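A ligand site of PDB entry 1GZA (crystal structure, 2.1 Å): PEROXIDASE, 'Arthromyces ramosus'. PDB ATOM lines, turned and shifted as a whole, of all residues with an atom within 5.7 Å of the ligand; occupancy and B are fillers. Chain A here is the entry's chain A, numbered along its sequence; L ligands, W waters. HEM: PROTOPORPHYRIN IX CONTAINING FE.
An iron atom (FE) of the ligand is bound by a ring nitrogen (NE2) of His 184 (2.1 Å).
The backbone NH (N) of Gly 191 lies within hydrogen-bond range of an oxygen (O2A) of the ligand.
N of Glu 190 lies within hydrogen-bond range of O1A of the ligand (2.8 Å).
An oxygen (O2D) of the ligand sits at hydrogen-bond distance from the side-chain hydroxyl (OG) of Ser 188 (2.9 Å).
An oxygen (O1A) of the ligand lies within salt-bridge range of the guanidinium group of Arg 52 (3.9 Å).
An oxygen (O2D) of the ligand is in hydrogen-bond range of the backbone NH of Ser 188 (2.8 Å).
The side-chain carboxylate of Glu 190 lies within salt-bridge range of the side-chain amino group of Lys 49 (2.8 Å).
SD of Met 243 lies within hydrogen-bond range of OG of Ser 245, at 3.7 Å.
The backbone NH of Leu 201 is in hydrogen-bond range of the backbone carbonyl oxygen of Ala 187 (2.9 Å).
The backbone NH of Ser 245 lies within hydrogen-bond range of the backbone carbonyl oxygen of Pro 156, 3.3 Å away.
The side-chain amide oxygen (OE1) of Gln 189 sits at hydrogen-bond distance from the backbone NH (N) of Leu 192 (2.8 Å).
CD of Arg 48 touches O2D of the ligand, at 3.0 Å.
CD of Lys 49 touches O1D of the ligand (3.8 Å).
Leu 51 touches the ligand (O to CAC, 3.3 Å).
Phe 55 touches the ligand.
Pro 154 touches the ligand (O to CMB, 3.8 Å).
Gly 155 touches the ligand (C to CMB, 3.6 Å).
Pro 156 touches the ligand.
CG2 of Ile 163 touches CBB of the ligand, at 3.8 Å.
Leu 180 touches the ligand (O to CMC, 3.8 Å).
Leu 181 touches the ligand (CD1 to CHC, 3.6 Å).
Ala 183 touches the ligand (CB to CBC, 3.4 Å).
Leu 186 touches the ligand.
Ala 187 touches the ligand.
Gln 189 touches the ligand.
N of Leu 192 touches O2A of the ligand (3.8 Å).
SD of Met 243 touches CHB of the ligand, at 3.6 Å.
Ser 245 touches the ligand (OG to CMB, 3.7 Å).
Within 4 Å of the ligand: Arg 48, Lys 49, Leu 51, Arg 52, Phe 55, Pro 154, Gly 155, Pro 156, Ile 163, Leu 180, Leu 181, Ala 183, His 184, Leu 186, Ala 187, Ser 188, Gln 189, Glu 190, Gly 191, Leu 192, Met 243 and Ser 245.
The nearest printed residue that does not touch the ligand is Met 277 (4.02 Å).
Water W1 lies within hydrogen-bond range of an oxygen (O1D) of the ligand (2.7 Å), the side-chain hydroxyl (OG) of Ser 45 (2.8 Å), the side-chain carboxylate (OE2) of Glu 190 (2.9 Å) and the guanidinium group (NH1) of Arg 48 (3.0 Å).
Water W4 lies within hydrogen-bond range of an oxygen (O1A) of the ligand (2.7 Å), the guanidinium group (NH1) of Arg 52 (2.8 Å) and the side-chain amino group (NZ) of Lys 49 (2.9 Å).
Water W6 bridges an oxygen (O1A) of the ligand (3.0 Å) and the guanidinium group (NH1) of Arg 52 (3.2 Å).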
ATOM      1  N   SER A  45       7.961 -12.324  15.313  1.00  0.00           N
ATOM      2  CA  SER A  45       6.555 -12.235  14.959  1.00  0.00           C
ATOM      3  C   SER A  45       5.723 -11.145  15.666  1.00  0.00           C
ATOM      4  O   SER A  45       4.932 -10.540  14.948  1.00  0.00           O
ATOM      5  CB  SER A  45       5.996 -13.655  15.179  1.00  0.00           C
ATOM      6  OG  SER A  45       4.626 -13.734  14.799  1.00  0.00           O
ATOM      7  N   VAL A  47       6.419  -8.055  16.340  1.00  0.00           N
ATOM      8  CA  VAL A  47       6.589  -6.789  15.623  1.00  0.00           C
ATOM      9  C   VAL A  47       5.838  -6.853  14.279  1.00  0.00           C
ATOM     10  O   VAL A  47       5.141  -5.944  13.845  1.00  0.00           O
ATOM     11  CB  VAL A  47       8.088  -6.500  15.311  1.00  0.00           C
ATOM     12  CG1 VAL A  47       8.167  -5.163  14.625  1.00  0.00           C
ATOM     13  CG2 VAL A  47       8.936  -6.443  16.553  1.00  0.00           C
ATOM     14  N   ARG A  48       5.924  -7.966  13.573  1.00  0.00           N
ATOM     15  CA  ARG A  48       5.288  -8.124  12.268  1.00  0.00           C
ATOM     16  C   ARG A  48       3.797  -8.119  12.350  1.00  0.00           C
ATOM     17  O   ARG A  48       3.145  -7.524  11.519  1.00  0.00           O
ATOM     18  CB  ARG A  48       5.767  -9.400  11.650  1.00  0.00           C
ATOM     19  CG  ARG A  48       7.261  -9.522  11.462  1.00  0.00           C
ATOM     20  CD  ARG A  48       7.256 -10.796  10.691  1.00  0.00           C
ATOM     21  NE  ARG A  48       8.386 -11.465  11.143  1.00  0.00           N
ATOM     22  CZ  ARG A  48       8.425 -12.666  11.631  1.00  0.00           C
ATOM     23  NH1 ARG A  48       7.415 -13.507  11.768  1.00  0.00           N
ATOM     24  NH2 ARG A  48       9.593 -12.896  12.142  1.00  0.00           N
ATOM     25  N   LYS A  49       3.185  -8.724  13.347  1.00  0.00           N
ATOM     26  CA  LYS A  49       1.749  -8.708  13.528  1.00  0.00           C
ATOM     27  C   LYS A  49       1.348  -7.293  13.905  1.00  0.00           C
ATOM     28  O   LYS A  49       0.339  -6.826  13.398  1.00  0.00           O
ATOM     29  CB  LYS A  49       1.319  -9.631  14.648  1.00  0.00           C
ATOM     30  CG  LYS A  49       1.598 -11.130  14.531  1.00  0.00           C
ATOM     31  CD  LYS A  49       0.789 -11.694  13.406  1.00  0.00           C
ATOM     32  CE  LYS A  49       0.776 -13.168  13.541  1.00  0.00           C
ATOM     33  NZ  LYS A  49       0.037 -13.757  12.439  1.00  0.00           N
ATOM     34  N   LEU A  51       2.718  -4.498  12.913  1.00  0.00           N
ATOM     35  CA  LEU A  51       2.798  -3.709  11.703  1.00  0.00           C
ATOM     36  C   LEU A  51       1.575  -3.972  10.816  1.00  0.00           C
ATOM     37  O   LEU A  51       1.102  -3.046  10.166  1.00  0.00           O
ATOM     38  CB  LEU A  51       4.107  -4.015  10.991  1.00  0.00           C
ATOM     39  CG  LEU A  51       5.362  -3.320  11.598  1.00  0.00           C
ATOM     40  CD1 LEU A  51       6.617  -3.816  10.917  1.00  0.00           C
ATOM     41  CD2 LEU A  51       5.277  -1.810  11.387  1.00  0.00           C
ATOM     42  N   ARG A  52       1.002  -5.203  10.795  1.00  0.00           N
ATOM     43  CA  ARG A  52      -0.210  -5.510  10.076  1.00  0.00           C
ATOM     44  C   ARG A  52      -1.345  -4.792  10.782  1.00  0.00           C
ATOM     45  O   ARG A  52      -2.159  -4.166  10.118  1.00  0.00           O
ATOM     46  CB  ARG A  52      -0.590  -6.957  10.114  1.00  0.00           C
ATOM     47  CG  ARG A  52      -0.007  -7.756   8.996  1.00  0.00           C
ATOM     48  CD  ARG A  52      -0.428  -9.210   9.103  1.00  0.00           C
ATOM     49  NE  ARG A  52      -1.832  -9.424   8.762  1.00  0.00           N
ATOM     50  CZ  ARG A  52      -2.502 -10.502   9.194  1.00  0.00           C
ATOM     51  NH1 ARG A  52      -1.918 -11.432   9.965  1.00  0.00           N
ATOM     52  NH2 ARG A  52      -3.760 -10.658   8.842  1.00  0.00           N
ATOM     53  N   VAL A  54      -1.349  -1.991  12.712  1.00  0.00           N
ATOM     54  CA  VAL A  54      -1.383  -0.540  12.623  1.00  0.00           C
ATOM     55  C   VAL A  54      -1.993  -0.086  11.296  1.00  0.00           C
ATOM     56  O   VAL A  54      -2.836   0.833  11.268  1.00  0.00           O
ATOM     57  CB  VAL A  54       0.075  -0.103  12.874  1.00  0.00           C
ATOM     58  CG1 VAL A  54       1.020  -0.271  11.703  1.00  0.00           C
ATOM     59  CG2 VAL A  54      -0.043   1.348  13.295  1.00  0.00           C
ATOM     60  N   PHE A  55      -1.669  -0.776  10.204  1.00  0.00           N
ATOM     61  CA  PHE A  55      -2.202  -0.502   8.900  1.00  0.00           C
ATOM     62  C   PHE A  55      -3.695  -0.790   8.918  1.00  0.00           C
ATOM     63  O   PHE A  55      -4.466   0.109   8.628  1.00  0.00           O
ATOM     64  CB  PHE A  55      -1.489  -1.383   7.854  1.00  0.00           C
ATOM     65  CG  PHE A  55      -2.027  -1.299   6.425  1.00  0.00           C
ATOM     66  CD1 PHE A  55      -2.381  -0.087   5.843  1.00  0.00           C
ATOM     67  CD2 PHE A  55      -2.165  -2.451   5.679  1.00  0.00           C
ATOM     68  CE1 PHE A  55      -2.864  -0.069   4.560  1.00  0.00           C
ATOM     69  CE2 PHE A  55      -2.654  -2.430   4.402  1.00  0.00           C
ATOM     70  CZ  PHE A  55      -3.005  -1.235   3.832  1.00  0.00           C
ATOM     71  N   PRO A 154      -7.092  -3.119   1.531  1.00  0.00           N
ATOM     72  CA  PRO A 154      -6.649  -3.719   0.282  1.00  0.00           C
ATOM     73  C   PRO A 154      -6.343  -5.200   0.498  1.00  0.00           C
ATOM     74  O   PRO A 154      -5.811  -5.564   1.556  1.00  0.00           O
ATOM     75  CB  PRO A 154      -5.430  -2.959  -0.106  1.00  0.00           C
ATOM     76  CG  PRO A 154      -5.649  -1.632   0.491  1.00  0.00           C
ATOM     77  CD  PRO A 154      -6.289  -1.939   1.838  1.00  0.00           C
ATOM     78  N   GLY A 155      -6.590  -6.069  -0.474  1.00  0.00           N
ATOM     79  CA  GLY A 155      -6.313  -7.477  -0.362  1.00  0.00           C
ATOM     80  C   GLY A 155      -5.246  -7.859  -1.349  1.00  0.00           C
ATOM     81  O   GLY A 155      -5.073  -7.160  -2.347  1.00  0.00           O
ATOM     82  N   PRO A 156      -4.527  -8.962  -1.195  1.00  0.00           N
ATOM     83  CA  PRO A 156      -3.467  -9.402  -2.087  1.00  0.00           C
ATOM     84  C   PRO A 156      -3.893  -9.816  -3.488  1.00  0.00           C
ATOM     85  O   PRO A 156      -3.050  -9.901  -4.387  1.00  0.00           O
ATOM     86  CB  PRO A 156      -2.788 -10.513  -1.334  1.00  0.00           C
ATOM     87  CG  PRO A 156      -3.952 -11.159  -0.634  1.00  0.00           C
ATOM     88  CD  PRO A 156      -4.702  -9.927  -0.128  1.00  0.00           C
ATOM     89  N   ILE A 163      -6.228  -1.167  -5.500  1.00  0.00           N
ATOM     90  CA  ILE A 163      -5.372  -0.752  -4.391  1.00  0.00           C
ATOM     91  C   ILE A 163      -5.133   0.745  -4.475  1.00  0.00           C
ATOM     92  O   ILE A 163      -5.339   1.410  -3.461  1.00  0.00           O
ATOM     93  CB  ILE A 163      -4.041  -1.517  -4.486  1.00  0.00           C
ATOM     94  CG1 ILE A 163      -4.341  -2.988  -4.244  1.00  0.00           C
ATOM     95  CG2 ILE A 163      -3.036  -0.977  -3.506  1.00  0.00           C
ATOM     96  CD1 ILE A 163      -3.132  -3.912  -4.468  1.00  0.00           C
ATOM     97  N   MET A 167      -6.455   3.229  -1.481  1.00  0.00           N
ATOM     98  CA  MET A 167      -5.417   3.984  -0.764  1.00  0.00           C
ATOM     99  C   MET A 167      -5.541   5.460  -1.038  1.00  0.00           C
ATOM    100  O   MET A 167      -5.334   6.262  -0.123  1.00  0.00           O
ATOM    101  CB  MET A 167      -4.003   3.506  -1.169  1.00  0.00           C
ATOM    102  CG  MET A 167      -3.570   2.112  -0.696  1.00  0.00           C
ATOM    103  SD  MET A 167      -3.636   1.859   1.093  1.00  0.00           S
ATOM    104  CE  MET A 167      -2.086   2.561   1.567  1.00  0.00           C
ATOM    105  N   VAL A 177       1.953   4.781  -1.350  1.00  0.00           N
ATOM    106  CA  VAL A 177       1.557   3.378  -1.242  1.00  0.00           C
ATOM    107  C   VAL A 177       2.860   2.619  -1.360  1.00  0.00           C
ATOM    108  O   VAL A 177       3.058   1.739  -0.538  1.00  0.00           O
ATOM    109  CB  VAL A 177       0.626   2.895  -2.406  1.00  0.00           C
ATOM    110  CG1 VAL A 177       0.312   1.401  -2.268  1.00  0.00           C
ATOM    111  CG2 VAL A 177      -0.630   3.718  -2.399  1.00  0.00           C
ATOM    112  N   LEU A 180       4.971   3.036   1.918  1.00  0.00           N
ATOM    113  CA  LEU A 180       4.369   2.322   3.041  1.00  0.00           C
ATOM    114  C   LEU A 180       4.695   0.836   2.989  1.00  0.00           C
ATOM    115  O   LEU A 180       4.842   0.139   4.008  1.00  0.00           O
ATOM    116  CB  LEU A 180       2.897   2.570   2.940  1.00  0.00           C
ATOM    117  CG  LEU A 180       2.070   3.088   4.075  1.00  0.00           C
ATOM    118  CD1 LEU A 180       2.796   4.024   4.994  1.00  0.00           C
ATOM    119  CD2 LEU A 180       0.907   3.766   3.404  1.00  0.00           C
ATOM    120  N   LEU A 181       4.852   0.313   1.778  1.00  0.00           N
ATOM    121  CA  LEU A 181       5.166  -1.083   1.572  1.00  0.00           C
ATOM    122  C   LEU A 181       6.565  -1.452   2.014  1.00  0.00           C
ATOM    123  O   LEU A 181       6.942  -2.625   1.901  1.00  0.00           O
ATOM    124  CB  LEU A 181       4.994  -1.429   0.122  1.00  0.00           C
ATOM    125  CG  LEU A 181       3.919  -2.390  -0.354  1.00  0.00           C
ATOM    126  CD1 LEU A 181       3.119  -2.994   0.767  1.00  0.00           C
ATOM    127  CD2 LEU A 181       3.015  -1.583  -1.240  1.00  0.00           C
ATOM    128  N   ALA A 183       7.335  -1.817   4.918  1.00  0.00           N
ATOM    129  CA  ALA A 183       7.077  -2.709   6.020  1.00  0.00           C
ATOM    130  C   ALA A 183       7.111  -4.167   5.585  1.00  0.00           C
ATOM    131  O   ALA A 183       7.367  -5.015   6.429  1.00  0.00           O
ATOM    132  CB  ALA A 183       5.738  -2.423   6.615  1.00  0.00           C
ATOM    133  N   HIS A 184       6.989  -4.547   4.311  1.00  0.00           N
ATOM    134  CA  HIS A 184       7.103  -5.928   3.887  1.00  0.00           C
ATOM    135  C   HIS A 184       8.577  -6.384   3.891  1.00  0.00           C
ATOM    136  O   HIS A 184       8.924  -7.517   3.530  1.00  0.00           O
ATOM    137  CB  HIS A 184       6.513  -6.144   2.486  1.00  0.00           C
ATOM    138  CG  HIS A 184       4.972  -6.257   2.451  1.00  0.00           C
ATOM    139  ND1 HIS A 184       4.221  -6.612   1.341  1.00  0.00           N
ATOM    140  CD2 HIS A 184       4.131  -6.114   3.547  1.00  0.00           C
ATOM    141  CE1 HIS A 184       2.962  -6.745   1.759  1.00  0.00           C
ATOM    142  NE2 HIS A 184       2.869  -6.451   3.013  1.00  0.00           N
ATOM    143  N   LEU A 186      10.038  -6.552   6.682  1.00  0.00           N
ATOM    144  CA  LEU A 186      10.014  -7.163   7.991  1.00  0.00           C
ATOM    145  C   LEU A 186       8.764  -8.032   7.960  1.00  0.00           C
ATOM    146  O   LEU A 186       7.819  -7.870   8.755  1.00  0.00           O
ATOM    147  CB  LEU A 186       9.976  -5.966   8.925  1.00  0.00           C
ATOM    148  CG  LEU A 186      11.110  -5.515   9.859  1.00  0.00           C
ATOM    149  CD1 LEU A 186      12.441  -5.768   9.280  1.00  0.00           C
ATOM    150  CD2 LEU A 186      10.928  -4.066  10.141  1.00  0.00           C
ATOM    151  N   ALA A 187       8.738  -9.059   7.112  1.00  0.00           N
ATOM    152  CA  ALA A 187       7.487  -9.782   6.902  1.00  0.00           C
ATOM    153  C   ALA A 187       7.428 -11.231   6.478  1.00  0.00           C
ATOM    154  O   ALA A 187       8.303 -11.701   5.756  1.00  0.00           O
ATOM    155  CB  ALA A 187       6.624  -9.056   5.849  1.00  0.00           C
ATOM    156  N   SER A 188       6.364 -11.921   6.800  1.00  0.00           N
ATOM    157  CA  SER A 188       6.200 -13.282   6.345  1.00  0.00           C
ATOM    158  C   SER A 188       4.705 -13.472   6.130  1.00  0.00           C
ATOM    159  O   SER A 188       3.914 -12.517   6.239  1.00  0.00           O
ATOM    160  CB  SER A 188       6.733 -14.246   7.384  1.00  0.00           C
ATOM    161  OG  SER A 188       5.933 -14.332   8.546  1.00  0.00           O
ATOM    162  N   GLN A 189       4.270 -14.645   5.659  1.00  0.00           N
ATOM    163  CA  GLN A 189       2.832 -14.873   5.559  1.00  0.00           C
ATOM    164  C   GLN A 189       2.567 -16.124   6.390  1.00  0.00           C
ATOM    165  O   GLN A 189       3.466 -16.975   6.513  1.00  0.00           O
ATOM    166  CB  GLN A 189       2.411 -15.098   4.080  1.00  0.00           C
ATOM    167  CG  GLN A 189       3.057 -16.300   3.415  1.00  0.00           C
ATOM    168  CD  GLN A 189       2.328 -17.621   3.633  1.00  0.00           C
ATOM    169  OE1 GLN A 189       1.121 -17.639   3.887  1.00  0.00           O
ATOM    170  NE2 GLN A 189       3.019 -18.750   3.568  1.00  0.00           N
ATOM    171  N   GLU A 190       1.373 -16.272   6.958  1.00  0.00           N
ATOM    172  CA  GLU A 190       1.010 -17.451   7.731  1.00  0.00           C
ATOM    173  C   GLU A 190      -0.276 -18.051   7.183  1.00  0.00           C
ATOM    174  O   GLU A 190      -0.424 -19.267   7.223  1.00  0.00           O
ATOM    175  CB  GLU A 190       0.761 -17.126   9.168  1.00  0.00           C
ATOM    176  CG  GLU A 190       2.027 -16.831   9.932  1.00  0.00           C
ATOM    177  CD  GLU A 190       1.838 -16.449  11.391  1.00  0.00           C
ATOM    178  OE1 GLU A 190       0.732 -16.466  11.905  1.00  0.00           O
ATOM    179  OE2 GLU A 190       2.834 -16.132  12.033  1.00  0.00           O
ATOM    180  N   GLY A 191      -1.171 -17.231   6.647  1.00  0.00           N
ATOM    181  CA  GLY A 191      -2.464 -17.698   6.193  1.00  0.00           C
ATOM    182  C   GLY A 191      -2.658 -17.714   4.699  1.00  0.00           C
ATOM    183  O   GLY A 191      -3.760 -18.049   4.249  1.00  0.00           O
ATOM    184  N   LEU A 192      -1.702 -17.385   3.845  1.00  0.00           N
ATOM    185  CA  LEU A 192      -1.921 -17.396   2.399  1.00  0.00           C
ATOM    186  C   LEU A 192      -1.601 -18.792   1.900  1.00  0.00           C
ATOM    187  O   LEU A 192      -2.230 -19.358   0.997  1.00  0.00           O
ATOM    188  CB  LEU A 192      -1.023 -16.340   1.803  1.00  0.00           C
ATOM    189  CG  LEU A 192      -1.582 -15.075   1.209  1.00  0.00           C
ATOM    190  CD1 LEU A 192      -2.939 -14.710   1.745  1.00  0.00           C
ATOM    191  CD2 LEU A 192      -0.546 -14.009   1.448  1.00  0.00           C
ATOM    192  N   LEU A 201       9.070 -12.646   3.081  1.00  0.00           N
ATOM    193  CA  LEU A 201       8.765 -11.916   1.865  1.00  0.00           C
ATOM    194  C   LEU A 201      10.071 -11.314   1.331  1.00  0.00           C
ATOM    195  O   LEU A 201      10.117 -10.839   0.197  1.00  0.00           O
ATOM    196  CB  LEU A 201       7.666 -10.895   2.220  1.00  0.00           C
ATOM    197  CG  LEU A 201       6.154 -11.231   1.968  1.00  0.00           C
ATOM    198  CD1 LEU A 201       5.716 -12.589   2.481  1.00  0.00           C
ATOM    199  CD2 LEU A 201       5.332 -10.174   2.660  1.00  0.00           C
ATOM    200  N   MET A 243       3.695 -12.437  -2.969  1.00  0.00           N
ATOM    201  CA  MET A 243       2.257 -12.275  -3.116  1.00  0.00           C
ATOM    202  C   MET A 243       1.997 -11.433  -4.352  1.00  0.00           C
ATOM    203  O   MET A 243       2.772 -10.550  -4.732  1.00  0.00           O
ATOM    204  CB  MET A 243       1.594 -11.610  -1.857  1.00  0.00           C
ATOM    205  CG  MET A 243       1.893 -10.174  -1.458  1.00  0.00           C
ATOM    206  SD  MET A 243       0.962  -9.594  -0.028  1.00  0.00           S
ATOM    207  CE  MET A 243       1.977 -10.473   1.113  1.00  0.00           C
ATOM    208  N   SER A 245      -0.066  -8.856  -5.249  1.00  0.00           N
ATOM    209  CA  SER A 245      -0.114  -7.418  -5.245  1.00  0.00           C
ATOM    210  C   SER A 245       1.286  -6.801  -5.260  1.00  0.00           C
ATOM    211  O   SER A 245       1.515  -5.816  -5.977  1.00  0.00           O
ATOM    212  CB  SER A 245      -0.913  -6.998  -4.008  1.00  0.00           C
ATOM    213  OG  SER A 245      -0.459  -7.585  -2.782  1.00  0.00           O
ATOM    214  N   LEU A 249       2.500  -4.445  -8.234  1.00  0.00           N
ATOM    215  CA  LEU A 249       2.899  -3.062  -7.950  1.00  0.00           C
ATOM    216  C   LEU A 249       4.331  -2.805  -8.318  1.00  0.00           C
ATOM    217  O   LEU A 249       4.643  -1.687  -8.700  1.00  0.00           O
ATOM    218  CB  LEU A 249       2.705  -2.684  -6.479  1.00  0.00           C
ATOM    219  CG  LEU A 249       1.267  -2.452  -6.004  1.00  0.00           C
ATOM    220  CD1 LEU A 249       1.152  -2.729  -4.520  1.00  0.00           C
ATOM    221  CD2 LEU A 249       0.840  -1.023  -6.370  1.00  0.00           C
ATOM    222  N   TYR A 273       9.583   6.092   4.267  1.00  0.00           N
ATOM    223  CA  TYR A 273       8.759   5.265   5.108  1.00  0.00           C
ATOM    224  C   TYR A 273       8.350   6.022   6.372  1.00  0.00           C
ATOM    225  O   TYR A 273       7.193   5.970   6.749  1.00  0.00           O
ATOM    226  CB  TYR A 273       9.523   3.989   5.448  1.00  0.00           C
ATOM    227  CG  TYR A 273       8.718   3.102   6.378  1.00  0.00           C
ATOM    228  CD1 TYR A 273       7.638   2.394   5.887  1.00  0.00           C
ATOM    229  CD2 TYR A 273       9.079   3.013   7.684  1.00  0.00           C
ATOM    230  CE1 TYR A 273       6.911   1.587   6.704  1.00  0.00           C
ATOM    231  CE2 TYR A 273       8.356   2.205   8.518  1.00  0.00           C
ATOM    232  CZ  TYR A 273       7.281   1.493   8.020  1.00  0.00           C
ATOM    233  OH  TYR A 273       6.606   0.629   8.852  1.00  0.00           O
ATOM    234  N   MET A 277       4.368   6.843   7.322  1.00  0.00           N
ATOM    235  CA  MET A 277       3.831   6.341   8.572  1.00  0.00           C
ATOM    236  C   MET A 277       3.349   7.457   9.442  1.00  0.00           C
ATOM    237  O   MET A 277       2.333   7.244  10.119  1.00  0.00           O
ATOM    238  CB  MET A 277       4.852   5.544   9.399  1.00  0.00           C
ATOM    239  CG  MET A 277       5.123   4.166   8.787  1.00  0.00           C
ATOM    240  SD  MET A 277       3.672   3.089   8.842  1.00  0.00           S
ATOM    241  CE  MET A 277       3.990   2.568  10.503  1.00  0.00           C
ATOM    242  N   MET A 280      -0.014   8.251   8.100  1.00  0.00           N
ATOM    243  CA  MET A 280      -0.951   7.207   8.390  1.00  0.00           C
ATOM    244  C   MET A 280      -1.330   7.194   9.848  1.00  0.00           C
ATOM    245  O   MET A 280      -2.441   6.769  10.160  1.00  0.00           O
ATOM    246  CB  MET A 280      -0.358   5.843   7.984  1.00  0.00           C
ATOM    247  CG  MET A 280      -1.420   4.771   8.163  1.00  0.00           C
ATOM    248  SD  MET A 280      -1.045   3.146   7.523  1.00  0.00           S
ATOM    249  CE  MET A 280       0.152   2.742   8.735  1.00  0.00           C
HETATM  250  CHA HEM L   1       1.762  -9.348   5.710  1.00  0.00           C
HETATM  251  CHB HEM L   1      -1.125  -7.733   2.203  1.00  0.00           C
HETATM  252  CHC HEM L   1       0.367  -3.243   3.026  1.00  0.00           C
HETATM  253  CHD HEM L   1       2.712  -4.805   6.891  1.00  0.00           C
HETATM  254  C1A HEM L   1       0.796  -9.272   4.728  1.00  0.00           C
HETATM  255  C2A HEM L   1      -0.022 -10.388   4.319  1.00  0.00           C
HETATM  256  C3A HEM L   1      -0.874  -9.935   3.362  1.00  0.00           C
HETATM  257  C4A HEM L   1      -0.557  -8.534   3.173  1.00  0.00           C
HETATM  258  CMA HEM L   1      -1.945 -10.712   2.635  1.00  0.00           C
HETATM  259  CAA HEM L   1       0.142 -11.797   4.853  1.00  0.00           C
HETATM  260  CBA HEM L   1      -0.538 -12.040   6.177  1.00  0.00           C
HETATM  261  CGA HEM L   1      -0.539 -13.487   6.589  1.00  0.00           C
HETATM  262  O1A HEM L   1       0.083 -13.833   7.566  1.00  0.00           O
HETATM  263  O2A HEM L   1      -1.144 -14.321   5.952  1.00  0.00           O
HETATM  264  C1B HEM L   1      -0.841  -6.388   2.008  1.00  0.00           C
HETATM  265  C2B HEM L   1      -1.467  -5.545   1.000  1.00  0.00           C
HETATM  266  C3B HEM L   1      -1.033  -4.257   1.242  1.00  0.00           C
HETATM  267  C4B HEM L   1      -0.118  -4.341   2.368  1.00  0.00           C
HETATM  268  CMB HEM L   1      -2.427  -6.028  -0.103  1.00  0.00           C
HETATM  269  CAB HEM L   1      -1.415  -3.059   0.607  1.00  0.00           C
HETATM  270  CBB HEM L   1      -1.123  -2.704  -0.770  1.00  0.00           C
HETATM  271  C1C HEM L   1       1.036  -3.289   4.214  1.00  0.00           C
HETATM  272  C2C HEM L   1       1.316  -2.121   4.997  1.00  0.00           C
HETATM  273  C3C HEM L   1       1.882  -2.553   6.146  1.00  0.00           C
HETATM  274  C4C HEM L   1       2.001  -3.993   6.017  1.00  0.00           C
HETATM  275  CMC HEM L   1       1.169  -0.673   4.520  1.00  0.00           C
HETATM  276  CAC HEM L   1       2.261  -1.834   7.271  1.00  0.00           C
HETATM  277  CBC HEM L   1       2.973  -0.562   7.312  1.00  0.00           C
HETATM  278  C1D HEM L   1       2.827  -6.188   6.794  1.00  0.00           C
HETATM  279  C2D HEM L   1       3.646  -7.022   7.635  1.00  0.00           C
HETATM  280  C3D HEM L   1       3.341  -8.287   7.296  1.00  0.00           C
HETATM  281  C4D HEM L   1       2.404  -8.248   6.234  1.00  0.00           C
HETATM  282  CMD HEM L   1       4.730  -6.536   8.594  1.00  0.00           C
HETATM  283  CAD HEM L   1       3.940  -9.546   7.874  1.00  0.00           C
HETATM  284  CBD HEM L   1       3.085 -10.244   8.917  1.00  0.00           C
HETATM  285  CGD HEM L   1       3.755 -11.430   9.558  1.00  0.00           C
HETATM  286  O1D HEM L   1       3.161 -12.053  10.431  1.00  0.00           O
HETATM  287  O2D HEM L   1       4.872 -11.748   9.191  1.00  0.00           O
HETATM  288  NA  HEM L   1       0.448  -8.120   4.036  1.00  0.00           N
HETATM  289  NB  HEM L   1       0.024  -5.645   2.827  1.00  0.00           N
HETATM  290  NC  HEM L   1       1.435  -4.439   4.846  1.00  0.00           N
HETATM  291  ND  HEM L   1       2.146  -6.943   5.869  1.00  0.00           N
HETATM  292 FE   HEM L   1       1.190  -6.309   4.289  1.00  0.00          FE
HETATM  293  O   HOH W   1       4.421 -13.764  12.021  1.00  0.00           O
HETATM  294  O   HOH W   2      -2.491  -6.166   4.922  1.00  0.00           O
HETATM  295  O   HOH W   3      -3.716 -14.013   5.069  1.00  0.00           O
HETATM  296  O   HOH W   4       0.605 -12.599   9.874  1.00  0.00           O
HETATM  297  O   HOH W   5      -4.481  -7.465   3.116  1.00  0.00           O
HETATM  298  O   HOH W   6      -2.118 -14.626   9.485  1.00  0.00           O
